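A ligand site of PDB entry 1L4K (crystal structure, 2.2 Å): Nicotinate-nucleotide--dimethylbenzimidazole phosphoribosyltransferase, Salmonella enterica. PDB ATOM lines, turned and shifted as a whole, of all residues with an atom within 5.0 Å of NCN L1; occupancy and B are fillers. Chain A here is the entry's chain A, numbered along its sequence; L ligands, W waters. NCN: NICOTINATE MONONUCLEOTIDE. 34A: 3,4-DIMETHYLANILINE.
The backbone NH of Ala 178 is in hydrogen-bond range of an oxygen (O3P) of NCN L1, 2.5 Å away. The side-chain hydroxyl (OG1) of Thr 180 sits at hydrogen-bond distance from an oxygen (O1P) of NCN L1, at 2.7 Å. O3' of NCN L1 sits at hydrogen-bond distance from O of Gly 176, 3.4 Å away. The side-chain hydroxyl of Ser 291 is in hydrogen-bond range of an oxygen (O7) of NCN L1 (2.6 Å). The backbone carbonyl oxygen (O) of Leu 315 sits close to a nitrogen (N1) of 34A L2 (3.5 Å). The side-chain carboxylate (OE1) of Glu 174 lies within hydrogen-bond range of an oxygen (O2') of NCN L1 (2.7 Å). The backbone NH (N) of Phe 265 lies within hydrogen-bond range of an oxygen (O7) of NCN L1 (3.0 Å). N of Ala 203 is in hydrogen-bond range of O2P of NCN L1, at 2.9 Å. O1P of NCN L1 sits at hydrogen-bond distance from N of Thr 180 (3.2 Å). N1 of 34A L2 sits at hydrogen-bond distance from OE2 of Glu 317 (2.8 Å). The backbone NH (N) of Gly 176 sits at hydrogen-bond distance from an oxygen (O3') of NCN L1. An oxygen (O2') of NCN L1 sits at hydrogen-bond distance from the backbone carbonyl oxygen (O) of Leu 315 (3.1 Å).
The side-chain amino group (NZ) of Lys 213 is in hydrogen-bond range of the side-chain hydroxyl (OG1) of Thr 180, 2.7 Å away. The side-chain hydroxyl (OG) of Ser 291 sits close to the backbone NH (N) of Glu 293 (3.2 Å). The backbone NH (N) of Glu 317 sits at hydrogen-bond distance from the backbone carbonyl oxygen (O) of Glu 174. The backbone NH (N) of Gly 202 sits at hydrogen-bond distance from the side-chain carboxylate (OE2) of Glu 293 (3.2 Å). ND2 of Asn 179 sits close to O of Gly 176 (3.3 Å). The side-chain amide nitrogen (ND2) of Asn 179 lies within hydrogen-bond range of the side-chain carboxylate (OE1) of Glu 174, 2.9 Å away.
N1 of NCN L1 lies close to O of Arg 314, 3.4 Å away. Merely in contact with NCN L1: Asn 179 (3.1 Å), Gly 316 (3.3 Å), Met 177 (3.4 Å), Ala 78 (3.5 Å), Leu 266 (3.5 Å), Gly 202 (3.6 Å), Glu 293 (3.6 Å), Gly 264 (3.7 Å) and Glu 317 (3.9 Å). Hydrophobic or aromatic side chains that line NCN L1: Ala 78, Met 177, Ala 203, Phe 265 and Leu 266. Of the 25 residues printed, 18 come within 4 Å of NCN L1.
Water W4 lies within hydrogen-bond range of O1P of NCN L1 (2.7 Å), OG1 of Thr 181 (2.8 Å), O of Val 77 (3.0 Å) and O of Ala 178 (3.2 Å). Water W1 lies within hydrogen-bond range of O2P of NCN L1 and O of Ala 203. Water W3 lies within hydrogen-bond range of the side-chain carboxylate (OD2) of Asp 263, an oxygen (O8) of NCN L1, the backbone NH (N) of Gly 316 and the backbone NH (N) of Gly 264. Water W2 lies within hydrogen-bond range of O of Gly 202 and OE2 of Glu 293.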
ATOM      1  N   VAL A  77     -23.780  11.593   1.441  1.00  0.00           N
ATOM      2  CA  VAL A  77     -23.570  10.495   2.408  1.00  0.00           C
ATOM      3  C   VAL A  77     -24.854   9.881   2.982  1.00  0.00           C
ATOM      4  O   VAL A  77     -24.795   8.913   3.742  1.00  0.00           O
ATOM      5  CB  VAL A  77     -22.638  10.943   3.604  1.00  0.00           C
ATOM      6  CG1 VAL A  77     -21.282  11.371   3.067  1.00  0.00           C
ATOM      7  CG2 VAL A  77     -23.282  12.087   4.405  1.00  0.00           C
ATOM      8  N   ALA A  78     -26.018  10.415   2.600  1.00  0.00           N
ATOM      9  CA  ALA A  78     -27.317   9.921   3.090  1.00  0.00           C
ATOM     10  C   ALA A  78     -28.396   9.883   2.002  1.00  0.00           C
ATOM     11  O   ALA A  78     -28.577  10.857   1.279  1.00  0.00           O
ATOM     12  CB  ALA A  78     -27.797  10.775   4.264  1.00  0.00           C
ATOM     13  N   GLU A 174     -31.455  10.441  19.256  1.00  0.00           N
ATOM     14  CA  GLU A 174     -31.309  11.525  18.285  1.00  0.00           C
ATOM     15  C   GLU A 174     -32.131  11.309  17.020  1.00  0.00           C
ATOM     16  O   GLU A 174     -32.752  10.269  16.819  1.00  0.00           O
ATOM     17  CB  GLU A 174     -29.838  11.673  17.883  1.00  0.00           C
ATOM     18  CG  GLU A 174     -29.124  10.336  17.621  1.00  0.00           C
ATOM     19  CD  GLU A 174     -29.866   9.457  16.624  1.00  0.00           C
ATOM     20  OE1 GLU A 174     -29.992   9.839  15.451  1.00  0.00           O
ATOM     21  OE2 GLU A 174     -30.332   8.360  17.026  1.00  0.00           O
ATOM     22  N   LEU A 175     -32.092  12.333  16.172  1.00  0.00           N
ATOM     23  CA  LEU A 175     -32.777  12.366  14.885  1.00  0.00           C
ATOM     24  C   LEU A 175     -32.027  13.396  14.043  1.00  0.00           C
ATOM     25  O   LEU A 175     -31.913  14.560  14.434  1.00  0.00           O
ATOM     26  CB  LEU A 175     -34.224  12.811  15.077  1.00  0.00           C
ATOM     27  CG  LEU A 175     -35.096  12.928  13.822  1.00  0.00           C
ATOM     28  CD1 LEU A 175     -35.242  11.526  13.191  1.00  0.00           C
ATOM     29  CD2 LEU A 175     -36.489  13.489  14.181  1.00  0.00           C
ATOM     30  N   GLY A 176     -31.493  12.951  12.906  1.00  0.00           N
ATOM     31  CA  GLY A 176     -30.760  13.840  12.022  1.00  0.00           C
ATOM     32  C   GLY A 176     -30.182  13.111  10.826  1.00  0.00           C
ATOM     33  O   GLY A 176     -29.273  12.296  10.958  1.00  0.00           O
ATOM     34  N   MET A 177     -30.715  13.398   9.645  1.00  0.00           N
ATOM     35  CA  MET A 177     -30.244  12.771   8.431  1.00  0.00           C
ATOM     36  C   MET A 177     -28.769  13.047   8.253  1.00  0.00           C
ATOM     37  O   MET A 177     -28.306  14.181   8.438  1.00  0.00           O
ATOM     38  CB  MET A 177     -31.050  13.277   7.233  1.00  0.00           C
ATOM     39  CG  MET A 177     -32.560  13.129   7.400  1.00  0.00           C
ATOM     40  SD  MET A 177     -33.055  11.426   7.762  1.00  0.00           S
ATOM     41  CE  MET A 177     -33.467  11.549   9.535  1.00  0.00           C
ATOM     42  N   ALA A 178     -28.029  12.005   7.895  1.00  0.00           N
ATOM     43  CA  ALA A 178     -26.578  12.030   7.682  1.00  0.00           C
ATOM     44  C   ALA A 178     -25.732  12.000   8.958  1.00  0.00           C
ATOM     45  O   ALA A 178     -24.499  12.048   8.861  1.00  0.00           O
ATOM     46  CB  ALA A 178     -26.188  13.271   6.843  1.00  0.00           C
ATOM     47  N   ASN A 179     -26.342  11.863  10.132  1.00  0.00           N
ATOM     48  CA  ASN A 179     -25.507  11.888  11.337  1.00  0.00           C
ATOM     49  C   ASN A 179     -24.563  10.710  11.605  1.00  0.00           C
ATOM     50  O   ASN A 179     -23.671  10.834  12.445  1.00  0.00           O
ATOM     51  CB  ASN A 179     -26.323  12.265  12.607  1.00  0.00           C
ATOM     52  CG  ASN A 179     -27.353  11.214  13.021  1.00  0.00           C
ATOM     53  OD1 ASN A 179     -27.367  10.106  12.518  1.00  0.00           O
ATOM     54  ND2 ASN A 179     -28.203  11.585  13.974  1.00  0.00           N
ATOM     55  N   THR A 180     -24.723   9.583  10.907  1.00  0.00           N
ATOM     56  CA  THR A 180     -23.778   8.486  11.135  1.00  0.00           C
ATOM     57  C   THR A 180     -22.413   8.818  10.523  1.00  0.00           C
ATOM     58  O   THR A 180     -21.439   8.095  10.740  1.00  0.00           O
ATOM     59  CB  THR A 180     -24.256   7.131  10.581  1.00  0.00           C
ATOM     60  OG1 THR A 180     -24.425   7.207   9.156  1.00  0.00           O
ATOM     61  CG2 THR A 180     -25.577   6.737  11.240  1.00  0.00           C
ATOM     62  N   THR A 181     -22.334   9.898   9.737  1.00  0.00           N
ATOM     63  CA  THR A 181     -21.057  10.306   9.147  1.00  0.00           C
ATOM     64  C   THR A 181     -20.188  11.001  10.225  1.00  0.00           C
ATOM     65  O   THR A 181     -19.049  10.611  10.455  1.00  0.00           O
ATOM     66  CB  THR A 181     -21.274  11.234   7.937  1.00  0.00           C
ATOM     67  OG1 THR A 181     -21.808  10.471   6.855  1.00  0.00           O
ATOM     68  CG2 THR A 181     -19.957  11.869   7.489  1.00  0.00           C
ATOM     69  N   ILE A 201     -23.535   1.595   6.864  1.00  0.00           N
ATOM     70  CA  ILE A 201     -24.557   2.017   5.903  1.00  0.00           C
ATOM     71  C   ILE A 201     -25.600   2.977   6.462  1.00  0.00           C
ATOM     72  O   ILE A 201     -26.525   3.371   5.757  1.00  0.00           O
ATOM     73  CB  ILE A 201     -25.280   0.812   5.300  1.00  0.00           C
ATOM     74  CG1 ILE A 201     -26.128   0.122   6.368  1.00  0.00           C
ATOM     75  CG2 ILE A 201     -24.281  -0.171   4.718  1.00  0.00           C
ATOM     76  CD1 ILE A 201     -27.136  -0.835   5.823  1.00  0.00           C
ATOM     77  N   GLY A 202     -25.471   3.366   7.729  1.00  0.00           N
ATOM     78  CA  GLY A 202     -26.451   4.284   8.284  1.00  0.00           C
ATOM     79  C   GLY A 202     -27.872   3.825   7.958  1.00  0.00           C
ATOM     80  O   GLY A 202     -28.210   2.649   8.127  1.00  0.00           O
ATOM     81  N   ALA A 203     -28.705   4.751   7.467  1.00  0.00           N
ATOM     82  CA  ALA A 203     -30.083   4.432   7.113  1.00  0.00           C
ATOM     83  C   ALA A 203     -30.192   3.925   5.664  1.00  0.00           C
ATOM     84  O   ALA A 203     -30.618   4.654   4.754  1.00  0.00           O
ATOM     85  CB  ALA A 203     -30.979   5.672   7.317  1.00  0.00           C
ATOM     86  N   LYS A 213     -18.482   7.839   1.300  1.00  0.00           N
ATOM     87  CA  LYS A 213     -18.700   8.154   2.718  1.00  0.00           C
ATOM     88  C   LYS A 213     -17.396   8.017   3.509  1.00  0.00           C
ATOM     89  O   LYS A 213     -17.103   8.843   4.373  1.00  0.00           O
ATOM     90  CB  LYS A 213     -19.810   7.245   3.318  1.00  0.00           C
ATOM     91  CG  LYS A 213     -20.263   7.614   4.739  1.00  0.00           C
ATOM     92  CD  LYS A 213     -21.502   6.804   5.180  1.00  0.00           C
ATOM     93  CE  LYS A 213     -21.778   6.942   6.676  1.00  0.00           C
ATOM     94  NZ  LYS A 213     -22.981   6.136   7.115  1.00  0.00           N
ATOM     95  N   ASP A 263     -28.189   4.488  23.596  1.00  0.00           N
ATOM     96  CA  ASP A 263     -29.044   3.923  22.539  1.00  0.00           C
ATOM     97  C   ASP A 263     -28.120   3.176  21.591  1.00  0.00           C
ATOM     98  O   ASP A 263     -27.495   2.197  21.986  1.00  0.00           O
ATOM     99  CB  ASP A 263     -29.831   5.047  21.799  1.00  0.00           C
ATOM    100  CG  ASP A 263     -30.828   4.497  20.725  1.00  0.00           C
ATOM    101  OD1 ASP A 263     -31.374   3.382  20.899  1.00  0.00           O
ATOM    102  OD2 ASP A 263     -31.074   5.203  19.718  1.00  0.00           O
ATOM    103  N   GLY A 264     -28.018   3.649  20.349  1.00  0.00           N
ATOM    104  CA  GLY A 264     -27.167   3.010  19.356  1.00  0.00           C
ATOM    105  C   GLY A 264     -25.839   3.691  19.017  1.00  0.00           C
ATOM    106  O   GLY A 264     -25.231   4.366  19.855  1.00  0.00           O
ATOM    107  N   PHE A 265     -25.412   3.522  17.766  1.00  0.00           N
ATOM    108  CA  PHE A 265     -24.146   4.055  17.272  1.00  0.00           C
ATOM    109  C   PHE A 265     -23.916   5.540  17.535  1.00  0.00           C
ATOM    110  O   PHE A 265     -22.837   5.941  17.960  1.00  0.00           O
ATOM    111  CB  PHE A 265     -23.995   3.761  15.767  1.00  0.00           C
ATOM    112  CG  PHE A 265     -22.619   4.039  15.226  1.00  0.00           C
ATOM    113  CD1 PHE A 265     -22.420   5.011  14.263  1.00  0.00           C
ATOM    114  CD2 PHE A 265     -21.516   3.334  15.703  1.00  0.00           C
ATOM    115  CE1 PHE A 265     -21.135   5.291  13.776  1.00  0.00           C
ATOM    116  CE2 PHE A 265     -20.234   3.594  15.227  1.00  0.00           C
ATOM    117  CZ  PHE A 265     -20.048   4.587  14.268  1.00  0.00           C
ATOM    118  N   LEU A 266     -24.918   6.372  17.265  1.00  0.00           N
ATOM    119  CA  LEU A 266     -24.766   7.794  17.517  1.00  0.00           C
ATOM    120  C   LEU A 266     -24.503   8.030  19.001  1.00  0.00           C
ATOM    121  O   LEU A 266     -23.639   8.824  19.355  1.00  0.00           O
ATOM    122  CB  LEU A 266     -26.009   8.573  17.080  1.00  0.00           C
ATOM    123  CG  LEU A 266     -26.390   8.581  15.586  1.00  0.00           C
ATOM    124  CD1 LEU A 266     -25.147   8.781  14.754  1.00  0.00           C
ATOM    125  CD2 LEU A 266     -27.067   7.277  15.192  1.00  0.00           C
ATOM    126  N   SER A 291     -25.933  -1.994  18.401  1.00  0.00           N
ATOM    127  CA  SER A 291     -26.258  -1.452  17.091  1.00  0.00           C
ATOM    128  C   SER A 291     -25.694  -2.263  15.910  1.00  0.00           C
ATOM    129  O   SER A 291     -24.547  -2.725  15.944  1.00  0.00           O
ATOM    130  CB  SER A 291     -25.762  -0.012  16.983  1.00  0.00           C
ATOM    131  OG  SER A 291     -26.034   0.520  15.695  1.00  0.00           O
ATOM    132  N   GLU A 293     -24.755  -1.129  13.251  1.00  0.00           N
ATOM    133  CA  GLU A 293     -23.840  -0.285  12.493  1.00  0.00           C
ATOM    134  C   GLU A 293     -22.450  -0.915  12.563  1.00  0.00           C
ATOM    135  O   GLU A 293     -22.030  -1.406  13.605  1.00  0.00           O
ATOM    136  CB  GLU A 293     -23.844   1.138  13.063  1.00  0.00           C
ATOM    137  CG  GLU A 293     -23.085   2.203  12.284  1.00  0.00           C
ATOM    138  CD  GLU A 293     -23.818   2.748  11.054  1.00  0.00           C
ATOM    139  OE1 GLU A 293     -23.275   3.662  10.422  1.00  0.00           O
ATOM    140  OE2 GLU A 293     -24.922   2.289  10.702  1.00  0.00           O
ATOM    141  N   MET A 313     -30.755  -3.729  15.790  1.00  0.00           N
ATOM    142  CA  MET A 313     -31.457  -2.473  15.543  1.00  0.00           C
ATOM    143  C   MET A 313     -30.517  -1.372  15.067  1.00  0.00           C
ATOM    144  O   MET A 313     -29.321  -1.355  15.422  1.00  0.00           O
ATOM    145  CB  MET A 313     -32.208  -2.035  16.799  1.00  0.00           C
ATOM    146  CG  MET A 313     -33.535  -2.736  16.957  1.00  0.00           C
ATOM    147  SD  MET A 313     -34.185  -2.717  18.637  1.00  0.00           S
ATOM    148  CE  MET A 313     -34.381  -0.974  18.948  1.00  0.00           C
ATOM    149  N   ARG A 314     -31.063  -0.471  14.258  1.00  0.00           N
ATOM    150  CA  ARG A 314     -30.291   0.642  13.691  1.00  0.00           C
ATOM    151  C   ARG A 314     -31.239   1.783  13.294  1.00  0.00           C
ATOM    152  O   ARG A 314     -31.023   2.461  12.293  1.00  0.00           O
ATOM    153  CB  ARG A 314     -29.518   0.149  12.454  1.00  0.00           C
ATOM    154  CG  ARG A 314     -30.375  -0.574  11.428  1.00  0.00           C
ATOM    155  CD  ARG A 314     -29.513  -1.206  10.350  1.00  0.00           C
ATOM    156  NE  ARG A 314     -30.251  -2.025   9.384  1.00  0.00           N
ATOM    157  CZ  ARG A 314     -31.055  -1.544   8.434  1.00  0.00           C
ATOM    158  NH1 ARG A 314     -31.261  -0.245   8.306  1.00  0.00           N
ATOM    159  NH2 ARG A 314     -31.635  -2.396   7.583  1.00  0.00           N
ATOM    160  N   LEU A 315     -32.285   1.994  14.067  1.00  0.00           N
ATOM    161  CA  LEU A 315     -33.233   3.057  13.789  1.00  0.00           C
ATOM    162  C   LEU A 315     -32.794   4.386  14.405  1.00  0.00           C
ATOM    163  O   LEU A 315     -32.917   5.426  13.774  1.00  0.00           O
ATOM    164  CB  LEU A 315     -34.611   2.682  14.332  1.00  0.00           C
ATOM    165  CG  LEU A 315     -35.684   3.784  14.407  1.00  0.00           C
ATOM    166  CD1 LEU A 315     -35.999   4.333  13.012  1.00  0.00           C
ATOM    167  CD2 LEU A 315     -36.944   3.227  15.059  1.00  0.00           C
ATOM    168  N   GLY A 316     -32.277   4.333  15.627  1.00  0.00           N
ATOM    169  CA  GLY A 316     -31.890   5.542  16.313  1.00  0.00           C
ATOM    170  C   GLY A 316     -33.110   6.009  17.119  1.00  0.00           C
ATOM    171  O   GLY A 316     -33.936   5.170  17.537  1.00  0.00           O
ATOM    172  N   GLU A 317     -33.218   7.312  17.347  1.00  0.00           N
ATOM    173  CA  GLU A 317     -34.335   7.925  18.071  1.00  0.00           C
ATOM    174  C   GLU A 317     -34.356   7.643  19.572  1.00  0.00           C
ATOM    175  O   GLU A 317     -35.145   8.233  20.315  1.00  0.00           O
ATOM    176  CB  GLU A 317     -35.677   7.434  17.517  1.00  0.00           C
ATOM    177  CG  GLU A 317     -35.900   7.719  16.044  1.00  0.00           C
ATOM    178  CD  GLU A 317     -37.288   7.324  15.583  1.00  0.00           C
ATOM    179  OE1 GLU A 317     -38.129   6.987  16.463  1.00  0.00           O
ATOM    180  OE2 GLU A 317     -37.533   7.374  14.367  1.00  0.00           O
HETATM  181  P   NCN L   1     -27.731   8.327   7.864  1.00  0.00           P
HETATM  182  O1P NCN L   1     -26.372   8.782   8.286  1.00  0.00           O
HETATM  183  O2P NCN L   1     -27.634   7.365   6.719  1.00  0.00           O
HETATM  184  O3P NCN L   1     -28.647   9.600   7.399  1.00  0.00           O
HETATM  185  O5' NCN L   1     -28.465   7.619   9.090  1.00  0.00           O
HETATM  186  C5' NCN L   1     -28.654   8.365  10.326  1.00  0.00           C
HETATM  187  C4' NCN L   1     -30.023   8.424  10.641  1.00  0.00           C
HETATM  188  O4' NCN L   1     -30.588   7.073  10.751  1.00  0.00           O
HETATM  189  C3' NCN L   1     -30.359   9.132  11.947  1.00  0.00           C
HETATM  190  O3' NCN L   1     -31.573   9.948  11.890  1.00  0.00           O
HETATM  191  C2' NCN L   1     -30.425   7.936  12.960  1.00  0.00           C
HETATM  192  O2' NCN L   1     -31.510   8.176  13.901  1.00  0.00           O
HETATM  193  C1' NCN L   1     -30.612   6.672  12.098  1.00  0.00           C
HETATM  194  N1  NCN L   1     -29.607   5.543  12.330  1.00  0.00           N
HETATM  195  C6  NCN L   1     -28.961   4.870  11.229  1.00  0.00           C
HETATM  196  C5  NCN L   1     -28.068   3.852  11.627  1.00  0.00           C
HETATM  197  C4  NCN L   1     -27.776   3.448  12.972  1.00  0.00           C
HETATM  198  C3  NCN L   1     -28.511   4.221  13.973  1.00  0.00           C
HETATM  199  C2  NCN L   1     -29.401   5.242  13.654  1.00  0.00           C
HETATM  200  C7  NCN L   1     -28.092   3.678  15.332  1.00  0.00           C
HETATM  201  O7  NCN L   1     -27.307   2.788  15.565  1.00  0.00           O
HETATM  202  O8  NCN L   1     -28.757   4.365  16.281  1.00  0.00           O
HETATM  203  N1  34A L   2     -35.296   7.656  12.624  1.00  0.00           N
HETATM  204  C1  34A L   2     -35.500   7.728  11.202  1.00  0.00           C
HETATM  205  C2  34A L   2     -34.354   7.807  10.342  1.00  0.00           C
HETATM  206  C3  34A L   2     -34.511   7.882   8.991  1.00  0.00           C
HETATM  207  C4  34A L   2     -35.783   7.886   8.410  1.00  0.00           C
HETATM  208  C5  34A L   2     -36.938   7.816   9.266  1.00  0.00           C
HETATM  209  C6  34A L   2     -36.760   7.732  10.671  1.00  0.00           C
HETATM  210  C7  34A L   2     -35.924   7.962   6.891  1.00  0.00           C
HETATM  211  C8  34A L   2     -38.324   7.814   8.648  1.00  0.00           C
HETATM  212  O   HOH W   1     -28.841   6.895   4.280  1.00  0.00           O
HETATM  213  O   HOH W   2     -27.454   0.812  10.016  1.00  0.00           O
HETATM  214  O   HOH W   3     -30.522   3.030  18.081  1.00  0.00           O
HETATM  215  O   HOH W   4     -24.477   9.695   6.651  1.00  0.00           O
